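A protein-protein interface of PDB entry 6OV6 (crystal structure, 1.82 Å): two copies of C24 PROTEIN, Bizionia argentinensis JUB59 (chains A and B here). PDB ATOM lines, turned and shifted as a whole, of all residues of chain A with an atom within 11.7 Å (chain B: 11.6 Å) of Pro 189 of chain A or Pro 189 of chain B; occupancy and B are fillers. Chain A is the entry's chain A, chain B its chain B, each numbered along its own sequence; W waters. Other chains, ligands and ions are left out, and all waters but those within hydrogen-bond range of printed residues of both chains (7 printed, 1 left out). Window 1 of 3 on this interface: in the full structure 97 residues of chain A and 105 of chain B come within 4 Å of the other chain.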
ATOM      1  N   THR A 184       6.020 -32.932 -30.291  1.00  0.00           N
ATOM      2  CA  THR A 184       4.648 -33.025 -30.834  1.00  0.00           C
ATOM      3  C   THR A 184       4.572 -32.213 -32.101  1.00  0.00           C
ATOM      4  O   THR A 184       5.225 -31.163 -32.200  1.00  0.00           O
ATOM      5  CB  THR A 184       3.571 -32.508 -29.839  1.00  0.00           C
ATOM      6  OG1 THR A 184       3.848 -31.139 -29.516  1.00  0.00           O
ATOM      7  CG2 THR A 184       3.489 -33.324 -28.564  1.00  0.00           C
ATOM      8  N   LYS A 185       3.776 -32.680 -33.070  1.00  0.00           N
ATOM      9  CA  LYS A 185       3.612 -31.989 -34.341  1.00  0.00           C
ATOM     10  C   LYS A 185       2.860 -30.646 -34.106  1.00  0.00           C
ATOM     11  O   LYS A 185       3.169 -29.635 -34.735  1.00  0.00           O
ATOM     12  CB  LYS A 185       2.818 -32.897 -35.288  1.00  0.00           C
ATOM     13  CG  LYS A 185       2.730 -32.440 -36.730  1.00  0.00           C
ATOM     14  CD  LYS A 185       1.959 -33.446 -37.621  1.00  0.00           C
ATOM     15  CE  LYS A 185       2.729 -34.726 -37.961  1.00  0.00           C
ATOM     16  NZ  LYS A 185       2.162 -35.464 -39.150  1.00  0.00           N
ATOM     17  N   LYS A 186       1.848 -30.691 -33.203  1.00  0.00           N
ATOM     18  CA  LYS A 186       0.979 -29.556 -32.846  1.00  0.00           C
ATOM     19  C   LYS A 186       1.085 -29.232 -31.364  1.00  0.00           C
ATOM     20  O   LYS A 186       1.312 -30.119 -30.546  1.00  0.00           O
ATOM     21  CB  LYS A 186      -0.498 -29.917 -33.132  1.00  0.00           C
ATOM     22  CG  LYS A 186      -0.863 -30.316 -34.581  1.00  0.00           C
ATOM     23  CD  LYS A 186      -0.604 -29.262 -35.616  1.00  0.00           C
ATOM     24  CE  LYS A 186      -0.922 -29.842 -36.979  1.00  0.00           C
ATOM     25  NZ  LYS A 186      -1.193 -28.787 -37.986  1.00  0.00           N
ATOM     26  N   VAL A 187       0.835 -27.971 -31.007  1.00  0.00           N
ATOM     27  CA  VAL A 187       0.819 -27.511 -29.604  1.00  0.00           C
ATOM     28  C   VAL A 187      -0.240 -26.407 -29.480  1.00  0.00           C
ATOM     29  O   VAL A 187      -0.494 -25.707 -30.457  1.00  0.00           O
ATOM     30  CB  VAL A 187       2.229 -27.029 -29.175  1.00  0.00           C
ATOM     31  CG1 VAL A 187       2.693 -25.759 -29.913  1.00  0.00           C
ATOM     32  CG2 VAL A 187       2.431 -26.966 -27.672  1.00  0.00           C
ATOM     33  N   THR A 188      -0.837 -26.260 -28.306  1.00  0.00           N
ATOM     34  CA  THR A 188      -1.835 -25.214 -28.064  1.00  0.00           C
ATOM     35  C   THR A 188      -1.310 -24.322 -26.940  1.00  0.00           C
ATOM     36  O   THR A 188      -1.115 -24.810 -25.820  1.00  0.00           O
ATOM     37  CB  THR A 188      -3.216 -25.810 -27.761  1.00  0.00           C
ATOM     38  OG1 THR A 188      -3.650 -26.567 -28.872  1.00  0.00           O
ATOM     39  CG2 THR A 188      -4.277 -24.732 -27.452  1.00  0.00           C
ATOM     40  N   PRO A 189      -1.087 -23.007 -27.189  1.00  0.00           N
ATOM     41  CA  PRO A 189      -0.629 -22.132 -26.097  1.00  0.00           C
ATOM     42  C   PRO A 189      -1.696 -22.002 -25.019  1.00  0.00           C
ATOM     43  O   PRO A 189      -2.896 -22.085 -25.308  1.00  0.00           O
ATOM     44  CB  PRO A 189      -0.390 -20.780 -26.802  1.00  0.00           C
ATOM     45  CG  PRO A 189      -1.293 -20.806 -27.963  1.00  0.00           C
ATOM     46  CD  PRO A 189      -1.236 -22.244 -28.439  1.00  0.00           C
ATOM     47  N   SER A 190      -1.253 -21.868 -23.784  1.00  0.00           N
ATOM     48  CA  SER A 190      -2.157 -21.712 -22.641  1.00  0.00           C
ATOM     49  C   SER A 190      -1.550 -20.705 -21.698  1.00  0.00           C
ATOM     50  O   SER A 190      -0.350 -20.410 -21.767  1.00  0.00           O
ATOM     51  CB  SER A 190      -2.410 -23.065 -21.966  1.00  0.00           C
ATOM     52  OG  SER A 190      -1.228 -23.632 -21.427  1.00  0.00           O
ATOM     53  N   GLY A 191      -2.380 -20.149 -20.825  1.00  0.00           N
ATOM     54  CA  GLY A 191      -1.897 -19.185 -19.857  1.00  0.00           C
ATOM     55  C   GLY A 191      -3.023 -18.636 -19.016  1.00  0.00           C
ATOM     56  O   GLY A 191      -4.174 -19.032 -19.182  1.00  0.00           O
ATOM     57  N   ASN A 192      -2.675 -17.707 -18.147  1.00  0.00           N
ATOM     58  CA  ASN A 192      -3.605 -17.121 -17.180  1.00  0.00           C
ATOM     59  C   ASN A 192      -3.613 -15.618 -17.207  1.00  0.00           C
ATOM     60  O   ASN A 192      -2.616 -14.983 -17.549  1.00  0.00           O
ATOM     61  CB  ASN A 192      -3.213 -17.589 -15.776  1.00  0.00           C
ATOM     62  CG  ASN A 192      -3.410 -19.075 -15.597  1.00  0.00           C
ATOM     63  OD1 ASN A 192      -4.542 -19.573 -15.554  1.00  0.00           O
ATOM     64  ND2 ASN A 192      -2.308 -19.814 -15.571  1.00  0.00           N
ATOM     65  N   LEU A 193      -4.742 -15.046 -16.770  1.00  0.00           N
ATOM     66  CA  LEU A 193      -4.921 -13.601 -16.664  1.00  0.00           C
ATOM     67  C   LEU A 193      -5.045 -13.233 -15.194  1.00  0.00           C
ATOM     68  O   LEU A 193      -5.622 -14.003 -14.413  1.00  0.00           O
ATOM     69  CB  LEU A 193      -6.214 -13.166 -17.392  1.00  0.00           C
ATOM     70  CG  LEU A 193      -6.245 -13.180 -18.946  1.00  0.00           C
ATOM     71  CD1 LEU A 193      -5.052 -12.522 -19.535  1.00  0.00           C
ATOM     72  CD2 LEU A 193      -6.299 -14.603 -19.528  1.00  0.00           C
ATOM     73  N   THR A 255     -10.859 -16.401 -18.867  1.00  0.00           N
ATOM     74  CA  THR A 255     -10.196 -17.655 -19.224  1.00  0.00           C
ATOM     75  C   THR A 255      -9.659 -17.475 -20.647  1.00  0.00           C
ATOM     76  O   THR A 255     -10.380 -17.025 -21.524  1.00  0.00           O
ATOM     77  CB  THR A 255     -11.185 -18.839 -19.136  1.00  0.00           C
ATOM     78  OG1 THR A 255     -11.512 -19.014 -17.755  1.00  0.00           O
ATOM     79  CG2 THR A 255     -10.596 -20.170 -19.706  1.00  0.00           C
ATOM     80  N   PHE A 256      -8.415 -17.874 -20.861  1.00  0.00           N
ATOM     81  CA  PHE A 256      -7.793 -17.851 -22.173  1.00  0.00           C
ATOM     82  C   PHE A 256      -7.950 -19.239 -22.796  1.00  0.00           C
ATOM     83  O   PHE A 256      -7.625 -20.233 -22.132  1.00  0.00           O
ATOM     84  CB  PHE A 256      -6.290 -17.505 -22.041  1.00  0.00           C
ATOM     85  CG  PHE A 256      -5.541 -17.557 -23.363  1.00  0.00           C
ATOM     86  CD1 PHE A 256      -5.632 -16.508 -24.277  1.00  0.00           C
ATOM     87  CD2 PHE A 256      -4.751 -18.652 -23.688  1.00  0.00           C
ATOM     88  CE1 PHE A 256      -4.933 -16.550 -25.492  1.00  0.00           C
ATOM     89  CE2 PHE A 256      -4.053 -18.699 -24.902  1.00  0.00           C
ATOM     90  CZ  PHE A 256      -4.175 -17.664 -25.814  1.00  0.00           C
ATOM     91  N   THR A 257      -8.413 -19.300 -24.052  1.00  0.00           N
ATOM     92  CA  THR A 257      -8.536 -20.537 -24.832  1.00  0.00           C
ATOM     93  C   THR A 257      -7.636 -20.378 -26.058  1.00  0.00           C
ATOM     94  O   THR A 257      -7.972 -19.613 -26.959  1.00  0.00           O
ATOM     95  CB  THR A 257     -10.009 -20.859 -25.188  1.00  0.00           C
ATOM     96  OG1 THR A 257     -10.729 -21.065 -23.965  1.00  0.00           O
ATOM     97  CG2 THR A 257     -10.145 -22.116 -26.064  1.00  0.00           C
ATOM     98  N   GLY A 258      -6.503 -21.077 -26.083  1.00  0.00           N
ATOM     99  CA  GLY A 258      -5.574 -20.954 -27.203  1.00  0.00           C
ATOM    100  C   GLY A 258      -6.015 -21.672 -28.457  1.00  0.00           C
ATOM    101  O   GLY A 258      -6.806 -22.621 -28.403  1.00  0.00           O
ATOM    102  N   ASN A 259      -5.487 -21.227 -29.624  1.00  0.00           N
ATOM    103  CA  ASN A 259      -5.726 -21.898 -30.894  1.00  0.00           C
ATOM    104  C   ASN A 259      -4.520 -22.823 -31.121  1.00  0.00           C
ATOM    105  O   ASN A 259      -3.408 -22.437 -30.806  1.00  0.00           O
ATOM    106  CB  ASN A 259      -5.782 -20.902 -32.046  1.00  0.00           C
ATOM    107  CG  ASN A 259      -6.984 -19.981 -31.972  1.00  0.00           C
ATOM    108  OD1 ASN A 259      -6.880 -18.758 -32.138  1.00  0.00           O
ATOM    109  ND2 ASN A 259      -8.129 -20.554 -31.675  1.00  0.00           N
ATOM    110  N   GLN A 260      -4.748 -24.002 -31.689  1.00  0.00           N
ATOM    111  CA  GLN A 260      -3.668 -24.954 -31.985  1.00  0.00           C
ATOM    112  C   GLN A 260      -2.701 -24.338 -33.015  1.00  0.00           C
ATOM    113  O   GLN A 260      -3.116 -23.627 -33.920  1.00  0.00           O
ATOM    114  CB  GLN A 260      -4.246 -26.259 -32.523  1.00  0.00           C
ATOM    115  CG  GLN A 260      -3.192 -27.365 -32.706  1.00  0.00           C
ATOM    116  CD  GLN A 260      -3.866 -28.685 -32.987  1.00  0.00           C
ATOM    117  OE1 GLN A 260      -4.426 -28.893 -34.065  1.00  0.00           O
ATOM    118  NE2 GLN A 260      -3.867 -29.581 -32.000  1.00  0.00           N
ATOM    119  N   GLN A 261      -1.402 -24.603 -32.853  1.00  0.00           N
ATOM    120  CA  GLN A 261      -0.401 -24.109 -33.781  1.00  0.00           C
ATOM    121  C   GLN A 261       0.526 -25.262 -34.190  1.00  0.00           C
ATOM    122  O   GLN A 261       0.586 -26.287 -33.505  1.00  0.00           O
ATOM    123  CB  GLN A 261       0.361 -22.918 -33.199  1.00  0.00           C
ATOM    124  CG  GLN A 261       1.224 -23.243 -32.017  1.00  0.00           C
ATOM    125  CD  GLN A 261       1.708 -22.008 -31.284  1.00  0.00           C
ATOM    126  OE1 GLN A 261       0.987 -21.024 -31.098  1.00  0.00           O
ATOM    127  NE2 GLN A 261       2.950 -22.038 -30.831  1.00  0.00           N
ATOM    128  N   ASP A 262       1.175 -25.112 -35.331  1.00  0.00           N
ATOM    129  CA  ASP A 262       2.095 -26.105 -35.885  1.00  0.00           C
ATOM    130  C   ASP A 262       3.481 -25.888 -35.240  1.00  0.00           C
ATOM    131  O   ASP A 262       4.089 -24.817 -35.348  1.00  0.00           O
ATOM    132  CB  ASP A 262       2.128 -25.999 -37.414  1.00  0.00           C
ATOM    133  CG  ASP A 262       2.785 -27.183 -38.103  1.00  0.00           C
ATOM    134  OD1 ASP A 262       3.775 -27.711 -37.563  1.00  0.00           O
ATOM    135  OD2 ASP A 262       2.321 -27.559 -39.199  1.00  0.00           O
ATOM    136  N   ASN A 263       3.948 -26.918 -34.528  1.00  0.00           N
ATOM    137  CA  ASN A 263       5.187 -26.871 -33.757  1.00  0.00           C
ATOM    138  C   ASN A 263       6.452 -27.103 -34.611  1.00  0.00           C
ATOM    139  O   ASN A 263       7.567 -27.010 -34.100  1.00  0.00           O
ATOM    140  CB  ASN A 263       5.095 -27.893 -32.622  1.00  0.00           C
ATOM    141  CG  ASN A 263       5.884 -27.544 -31.401  1.00  0.00           C
ATOM    142  OD1 ASN A 263       6.264 -26.397 -31.151  1.00  0.00           O
ATOM    143  ND2 ASN A 263       6.121 -28.543 -30.599  1.00  0.00           N
ATOM    144  N   THR B 184       7.373 -23.675 -40.106  1.00  0.00           N
ATOM    145  CA  THR B 184       7.694 -22.237 -40.115  1.00  0.00           C
ATOM    146  C   THR B 184       8.756 -21.950 -39.076  1.00  0.00           C
ATOM    147  O   THR B 184       8.811 -22.599 -38.029  1.00  0.00           O
ATOM    148  CB  THR B 184       6.433 -21.348 -39.830  1.00  0.00           C
ATOM    149  OG1 THR B 184       5.992 -21.601 -38.493  1.00  0.00           O
ATOM    150  CG2 THR B 184       5.249 -21.606 -40.800  1.00  0.00           C
ATOM    151  N   LYS B 185       9.585 -20.950 -39.346  1.00  0.00           N
ATOM    152  CA  LYS B 185      10.647 -20.532 -38.444  1.00  0.00           C
ATOM    153  C   LYS B 185      10.038 -19.883 -37.188  1.00  0.00           C
ATOM    154  O   LYS B 185      10.529 -20.078 -36.071  1.00  0.00           O
ATOM    155  CB  LYS B 185      11.517 -19.507 -39.172  1.00  0.00           C
ATOM    156  CG  LYS B 185      12.768 -19.095 -38.425  1.00  0.00           C
ATOM    157  CD  LYS B 185      13.604 -18.069 -39.225  1.00  0.00           C
ATOM    158  CE  LYS B 185      14.328 -18.628 -40.422  1.00  0.00           C
ATOM    159  NZ  LYS B 185      15.366 -17.674 -40.895  1.00  0.00           N
ATOM    160  N   LYS B 186       9.019 -19.038 -37.410  1.00  0.00           N
ATOM    161  CA  LYS B 186       8.385 -18.304 -36.327  1.00  0.00           C
ATOM    162  C   LYS B 186       6.905 -18.643 -36.277  1.00  0.00           C
ATOM    163  O   LYS B 186       6.348 -19.122 -37.244  1.00  0.00           O
ATOM    164  CB  LYS B 186       8.534 -16.785 -36.544  1.00  0.00           C
ATOM    165  CG  LYS B 186       9.925 -16.258 -36.880  1.00  0.00           C
ATOM    166  CD  LYS B 186      10.910 -16.392 -35.718  1.00  0.00           C
ATOM    167  CE  LYS B 186      12.154 -15.589 -35.996  1.00  0.00           C
ATOM    168  NZ  LYS B 186      13.027 -15.575 -34.814  1.00  0.00           N
ATOM    169  N   VAL B 187       6.265 -18.382 -35.145  1.00  0.00           N
ATOM    170  CA  VAL B 187       4.814 -18.583 -34.976  1.00  0.00           C
ATOM    171  C   VAL B 187       4.338 -17.506 -34.005  1.00  0.00           C
ATOM    172  O   VAL B 187       5.105 -17.070 -33.143  1.00  0.00           O
ATOM    173  CB  VAL B 187       4.379 -20.003 -34.463  1.00  0.00           C
ATOM    174  CG1 VAL B 187       4.457 -21.068 -35.534  1.00  0.00           C
ATOM    175  CG2 VAL B 187       5.114 -20.410 -33.192  1.00  0.00           C
ATOM    176  N   THR B 188       3.073 -17.111 -34.123  1.00  0.00           N
ATOM    177  CA  THR B 188       2.485 -16.138 -33.191  1.00  0.00           C
ATOM    178  C   THR B 188       1.314 -16.842 -32.484  1.00  0.00           C
ATOM    179  O   THR B 188       0.365 -17.245 -33.147  1.00  0.00           O
ATOM    180  CB  THR B 188       2.069 -14.851 -33.915  1.00  0.00           C
ATOM    181  OG1 THR B 188       3.252 -14.264 -34.477  1.00  0.00           O
ATOM    182  CG2 THR B 188       1.421 -13.835 -32.966  1.00  0.00           C
ATOM    183  N   PRO B 189       1.331 -16.982 -31.149  1.00  0.00           N
ATOM    184  CA  PRO B 189       0.193 -17.632 -30.481  1.00  0.00           C
ATOM    185  C   PRO B 189      -1.059 -16.749 -30.613  1.00  0.00           C
ATOM    186  O   PRO B 189      -0.955 -15.527 -30.687  1.00  0.00           O
ATOM    187  CB  PRO B 189       0.647 -17.736 -29.023  1.00  0.00           C
ATOM    188  CG  PRO B 189       1.607 -16.615 -28.850  1.00  0.00           C
ATOM    189  CD  PRO B 189       2.355 -16.585 -30.174  1.00  0.00           C
ATOM    190  N   SER B 190      -2.213 -17.390 -30.706  1.00  0.00           N
ATOM    191  CA  SER B 190      -3.481 -16.672 -30.799  1.00  0.00           C
ATOM    192  C   SER B 190      -4.482 -17.397 -29.911  1.00  0.00           C
ATOM    193  O   SER B 190      -4.298 -18.572 -29.577  1.00  0.00           O
ATOM    194  CB  SER B 190      -3.947 -16.610 -32.255  1.00  0.00           C
ATOM    195  OG  SER B 190      -4.227 -17.888 -32.802  1.00  0.00           O
ATOM    196  N   GLY B 191      -5.530 -16.696 -29.529  1.00  0.00           N
ATOM    197  CA  GLY B 191      -6.544 -17.323 -28.698  1.00  0.00           C
ATOM    198  C   GLY B 191      -7.627 -16.347 -28.344  1.00  0.00           C
ATOM    199  O   GLY B 191      -7.575 -15.182 -28.747  1.00  0.00           O
ATOM    200  N   ASN B 192      -8.589 -16.828 -27.585  1.00  0.00           N
ATOM    201  CA  ASN B 192      -9.753 -16.030 -27.194  1.00  0.00           C
ATOM    202  C   ASN B 192      -9.973 -15.979 -25.708  1.00  0.00           C
ATOM    203  O   ASN B 192      -9.547 -16.862 -24.975  1.00  0.00           O
ATOM    204  CB  ASN B 192     -10.993 -16.577 -27.895  1.00  0.00           C
ATOM    205  CG  ASN B 192     -10.926 -16.391 -29.385  1.00  0.00           C
ATOM    206  OD1 ASN B 192     -11.032 -15.279 -29.897  1.00  0.00           O
ATOM    207  ND2 ASN B 192     -10.692 -17.473 -30.104  1.00  0.00           N
ATOM    208  N   LEU B 193     -10.614 -14.907 -25.263  1.00  0.00           N
ATOM    209  CA  LEU B 193     -10.989 -14.745 -23.875  1.00  0.00           C
ATOM    210  C   LEU B 193     -12.492 -14.916 -23.775  1.00  0.00           C
ATOM    211  O   LEU B 193     -13.226 -14.495 -24.680  1.00  0.00           O
ATOM    212  CB  LEU B 193     -10.628 -13.353 -23.368  1.00  0.00           C
ATOM    213  CG  LEU B 193      -9.176 -13.021 -23.099  1.00  0.00           C
ATOM    214  CD1 LEU B 193      -9.128 -11.800 -22.291  1.00  0.00           C
ATOM    215  CD2 LEU B 193      -8.459 -14.079 -22.324  1.00  0.00           C
ATOM    216  N   THR B 255      -9.371  -8.509 -26.483  1.00  0.00           N
ATOM    217  CA  THR B 255      -8.708  -9.122 -27.631  1.00  0.00           C
ATOM    218  C   THR B 255      -7.295  -9.472 -27.188  1.00  0.00           C
ATOM    219  O   THR B 255      -6.612  -8.630 -26.605  1.00  0.00           O
ATOM    220  CB  THR B 255      -8.718  -8.177 -28.849  1.00  0.00           C
ATOM    221  OG1 THR B 255     -10.072  -8.014 -29.266  1.00  0.00           O
ATOM    222  CG2 THR B 255      -7.881  -8.726 -30.038  1.00  0.00           C
ATOM    223  N   PHE B 256      -6.857 -10.706 -27.483  1.00  0.00           N
ATOM    224  CA  PHE B 256      -5.495 -11.129 -27.211  1.00  0.00           C
ATOM    225  C   PHE B 256      -4.669 -10.889 -28.487  1.00  0.00           C
ATOM    226  O   PHE B 256      -5.077 -11.318 -29.566  1.00  0.00           O
ATOM    227  CB  PHE B 256      -5.451 -12.631 -26.840  1.00  0.00           C
ATOM    228  CG  PHE B 256      -4.043 -13.165 -26.645  1.00  0.00           C
ATOM    229  CD1 PHE B 256      -3.369 -12.964 -25.453  1.00  0.00           C
ATOM    230  CD2 PHE B 256      -3.418 -13.905 -27.646  1.00  0.00           C
ATOM    231  CE1 PHE B 256      -2.083 -13.475 -25.261  1.00  0.00           C
ATOM    232  CE2 PHE B 256      -2.119 -14.400 -27.470  1.00  0.00           C
ATOM    233  CZ  PHE B 256      -1.457 -14.183 -26.281  1.00  0.00           C
ATOM    234  N   THR B 257      -3.513 -10.237 -28.344  1.00  0.00           N
ATOM    235  CA  THR B 257      -2.568 -10.028 -29.455  1.00  0.00           C
ATOM    236  C   THR B 257      -1.267 -10.720 -29.031  1.00  0.00           C
ATOM    237  O   THR B 257      -0.571 -10.233 -28.149  1.00  0.00           O
ATOM    238  CB  THR B 257      -2.352  -8.511 -29.732  1.00  0.00           C
ATOM    239  OG1 THR B 257      -3.602  -7.938 -30.104  1.00  0.00           O
ATOM    240  CG2 THR B 257      -1.316  -8.254 -30.851  1.00  0.00           C
ATOM    241  N   GLY B 258      -0.948 -11.827 -29.664  1.00  0.00           N
ATOM    242  CA  GLY B 258       0.270 -12.558 -29.313  1.00  0.00           C
ATOM    243  C   GLY B 258       1.536 -11.921 -29.845  1.00  0.00           C
ATOM    244  O   GLY B 258       1.505 -11.190 -30.840  1.00  0.00           O
ATOM    245  N   ASN B 259       2.662 -12.199 -29.179  1.00  0.00           N
ATOM    246  CA  ASN B 259       3.988 -11.764 -29.622  1.00  0.00           C
ATOM    247  C   ASN B 259       4.562 -12.918 -30.425  1.00  0.00           C
ATOM    248  O   ASN B 259       4.344 -14.078 -30.061  1.00  0.00           O
ATOM    249  CB  ASN B 259       4.908 -11.489 -28.445  1.00  0.00           C
ATOM    250  CG  ASN B 259       4.475 -10.327 -27.589  1.00  0.00           C
ATOM    251  OD1 ASN B 259       4.487 -10.385 -26.356  1.00  0.00           O
ATOM    252  ND2 ASN B 259       4.077  -9.260 -28.228  1.00  0.00           N
ATOM    253  N   GLN B 260       5.269 -12.612 -31.526  1.00  0.00           N
ATOM    254  CA  GLN B 260       5.918 -13.670 -32.326  1.00  0.00           C
ATOM    255  C   GLN B 260       6.949 -14.423 -31.455  1.00  0.00           C
ATOM    256  O   GLN B 260       7.631 -13.837 -30.609  1.00  0.00           O
ATOM    257  CB  GLN B 260       6.638 -13.040 -33.531  1.00  0.00           C
ATOM    258  CG  GLN B 260       7.147 -14.072 -34.518  1.00  0.00           C
ATOM    259  CD  GLN B 260       7.592 -13.434 -35.796  1.00  0.00           C
ATOM    260  OE1 GLN B 260       8.639 -12.793 -35.841  1.00  0.00           O
ATOM    261  NE2 GLN B 260       6.832 -13.672 -36.855  1.00  0.00           N
ATOM    262  N   GLN B 261       7.059 -15.737 -31.674  1.00  0.00           N
ATOM    263  CA  GLN B 261       8.036 -16.533 -30.940  1.00  0.00           C
ATOM    264  C   GLN B 261       8.793 -17.417 -31.944  1.00  0.00           C
ATOM    265  O   GLN B 261       8.322 -17.658 -33.046  1.00  0.00           O
ATOM    266  CB  GLN B 261       7.368 -17.366 -29.821  1.00  0.00           C
ATOM    267  CG  GLN B 261       6.421 -18.439 -30.326  1.00  0.00           C
ATOM    268  CD  GLN B 261       5.530 -19.001 -29.249  1.00  0.00           C
ATOM    269  OE1 GLN B 261       5.045 -18.289 -28.372  1.00  0.00           O
ATOM    270  NE2 GLN B 261       5.276 -20.292 -29.323  1.00  0.00           N
ATOM    271  N   ASP B 262       9.956 -17.883 -31.534  1.00  0.00           N
ATOM    272  CA  ASP B 262      10.805 -18.734 -32.368  1.00  0.00           C
ATOM    273  C   ASP B 262      10.318 -20.204 -32.260  1.00  0.00           C
ATOM    274  O   ASP B 262      10.305 -20.788 -31.172  1.00  0.00           O
ATOM    275  CB  ASP B 262      12.256 -18.569 -31.914  1.00  0.00           C
ATOM    276  CG  ASP B 262      13.246 -19.044 -32.949  1.00  0.00           C
ATOM    277  OD1 ASP B 262      12.967 -20.064 -33.600  1.00  0.00           O
ATOM    278  OD2 ASP B 262      14.317 -18.422 -33.065  1.00  0.00           O
ATOM    279  N   ASN B 263       9.892 -20.777 -33.391  1.00  0.00           N
ATOM    280  CA  ASN B 263       9.334 -22.138 -33.439  1.00  0.00           C
ATOM    281  C   ASN B 263      10.423 -23.223 -33.488  1.00  0.00           C
ATOM    282  O   ASN B 263      10.101 -24.413 -33.527  1.00  0.00           O
ATOM    283  CB  ASN B 263       8.422 -22.243 -34.682  1.00  0.00           C
ATOM    284  CG  ASN B 263       7.355 -23.287 -34.582  1.00  0.00           C
ATOM    285  OD1 ASN B 263       6.929 -23.680 -33.488  1.00  0.00           O
ATOM    286  ND2 ASN B 263       6.851 -23.720 -35.712  1.00  0.00           N
HETATM  287  O   HOH W   1       8.242 -25.396 -32.308  1.00  0.00           O
HETATM  288  O   HOH W   2     -11.789 -18.678 -23.151  1.00  0.00           O
HETATM  289  O   HOH W   3       4.301 -23.531 -37.843  1.00  0.00           O
HETATM  290  O   HOH W   4      -9.689 -19.985 -29.151  1.00  0.00           O
HETATM  291  O   HOH W   5      10.325 -27.306 -33.879  1.00  0.00           O
HETATM  292  O   HOH W   6      -1.909 -20.274 -31.399  1.00  0.00           O
HETATM  293  O   HOH W   7      -8.456 -16.302 -32.078  1.00  0.00           O
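The backbone carbonyl oxygen (O) of Thr 184 of chain A lies within hydrogen-bond range of the side-chain amide nitrogen (ND2) of Asn 263 of chain A, at 3.2 Å.
The backbone carbonyl oxygen of Val 187 of chain A lies within hydrogen-bond range of the backbone NH of Gln 261 of chain A (2.8 Å).
O of Thr 184 of chain B lies within hydrogen-bond range of ND2 of Asn 263 of chain B (3.2 Å).
The backbone NH (N) of Asn 263 of chain B lies within hydrogen-bond range of the backbone carbonyl oxygen (O) of Lys 185 of chain B (2.8 Å).
Pro 189 of chain A touches Pro 189 of chain B (CG to CB, 3.8 Å).
CD2 of Leu 193 of chain B touches CD2 of Leu 193 of chain A (3.6 Å).
Leu 193 of chain B touches Thr 255 of chain A (CA to O, 3.3 Å).
Ser 190 of chain B touches Phe 256 of chain A.
Phe 256 of chain A touches Gly 191 of chain B (CE1 to CA, 3.7 Å).
Phe 256 of chain A touches Leu 193 of chain B (CA to CD2, 3.8 Å).
Phe 256 of chain A touches Phe 256 of chain B.
Thr 257 of chain A touches Gly 191 of chain B.
Ser 190 of chain B touches Gly 258 of chain A.
Pro 189 of chain B touches Gln 261 of chain A (CA to OE1, 3.5 Å).
The backbone carbonyl oxygen (O) of Asn 192 of chain B is in hydrogen-bond range of the backbone NH (N) of Thr 257 of chain A, 2.8 Å away.
The side-chain amide oxygen (OD1) of Asn 259 of chain A lies within hydrogen-bond range of the side-chain hydroxyl (OG) of Ser 190 of chain B (2.9 Å).
NE2 of Gln 261 of chain A sits close to NE2 of Gln 261 of chain B.
ND2 of Asn 263 of chain B lies within hydrogen-bond range of O of Asp 262 of chain A, at 3.0 Å.
The side-chain amide oxygen (OD1) of Asn 263 of chain B lies close to the backbone carbonyl oxygen (O) of Asn 263 of chain A (3.4 Å).
No residue of chain B comes within 4 Å of Thr 188 of chain A.
No residue of chain B comes within 4 Å of Ser 190 of chain A.
No residue of chain B comes within 4 Å of Gly 191 of chain A.
Gln 261 of chain A touches just these residues of chain B: Val 187 (3.6 Å), Pro 189 (3.5 Å) and Gln 261 (3.3 Å).
Of the printed residues of chain B, Asn 263 of chain A touches Asn 263.
Pro 189 of chain B touches just these residues of chain A: Pro 189 (3.8 Å) and Gln 261 (3.5 Å).
Ser 190 of chain B touches three residues of chain A.
Of the printed residues of chain A, Leu 193 of chain B touches Leu 193, Thr 255 and Phe 256.
No residue of chain A comes within 4 Å of Gly 258 of chain B.
Gln 261 of chain B touches just one residue of chain A: Gln 261 (3.3 Å).
The nearest residue of chain B that does not touch Pro 189 of chain A is Ser 190 of chain B (4.1 Å).
The nearest residue of chain A that does not touch Pro 189 of chain B is Phe 256 of chain A (5.8 Å).
The nearest printed residue of chain B that does not touch Asn 259 of chain A is Asn 192 of chain B (4.3 Å).
Phe 256 of chain A touches Ser 190 of chain B, but with the chains exchanged Ser 190 of chain A does not touch Phe 256 of chain B (7.8 Å).
Phe 256 of chain A touches Asn 192 of chain B, but with the chains exchanged Asn 192 of chain A does not touch Phe 256 of chain B (7.9 Å).
Phe 256 of chain A touches its own counterpart, Phe 256 of chain B.
Asn 263 of chain B touches its own counterpart, Asn 263 of chain A.
Positions printed for both chains: 184, 185, 186, 187, 188, 189, 190, 191, 192, 193, 255, 256, 257, 258, 259, 260, 261, 262 and 263.
Hydrophobic or aromatic side chains of chain A within 4 Å of the printed part of chain B: Pro 189, Leu 193 and Phe 256.
Among the printed residues, 20 pairs touch across the chains.
Among the printed residues, no Asp or Glu carboxylate lies within 4 Å of a Lys or Arg side-chain nitrogen of the other chain.
Water W6 lies within hydrogen-bond range of O of Asn 259 of chain A (2.7 Å), N of Ser 190 of chain B (3.0 Å) and OE1 of Gln 261 of chain A (3.0 Å).
Water W2 lies within hydrogen-bond range of the backbone carbonyl oxygen of Thr 255 of chain A (2.7 Å), the side-chain hydroxyl of Thr 257 of chain A (2.7 Å) and the backbone carbonyl oxygen of Asn 192 of chain B (3.4 Å).
Water W4 lies within hydrogen-bond range of O of Thr 257 of chain A (2.8 Å), ND2 of Asn 192 of chain B (2.9 Å) and ND2 of Asn 259 of chain A (3.0 Å).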
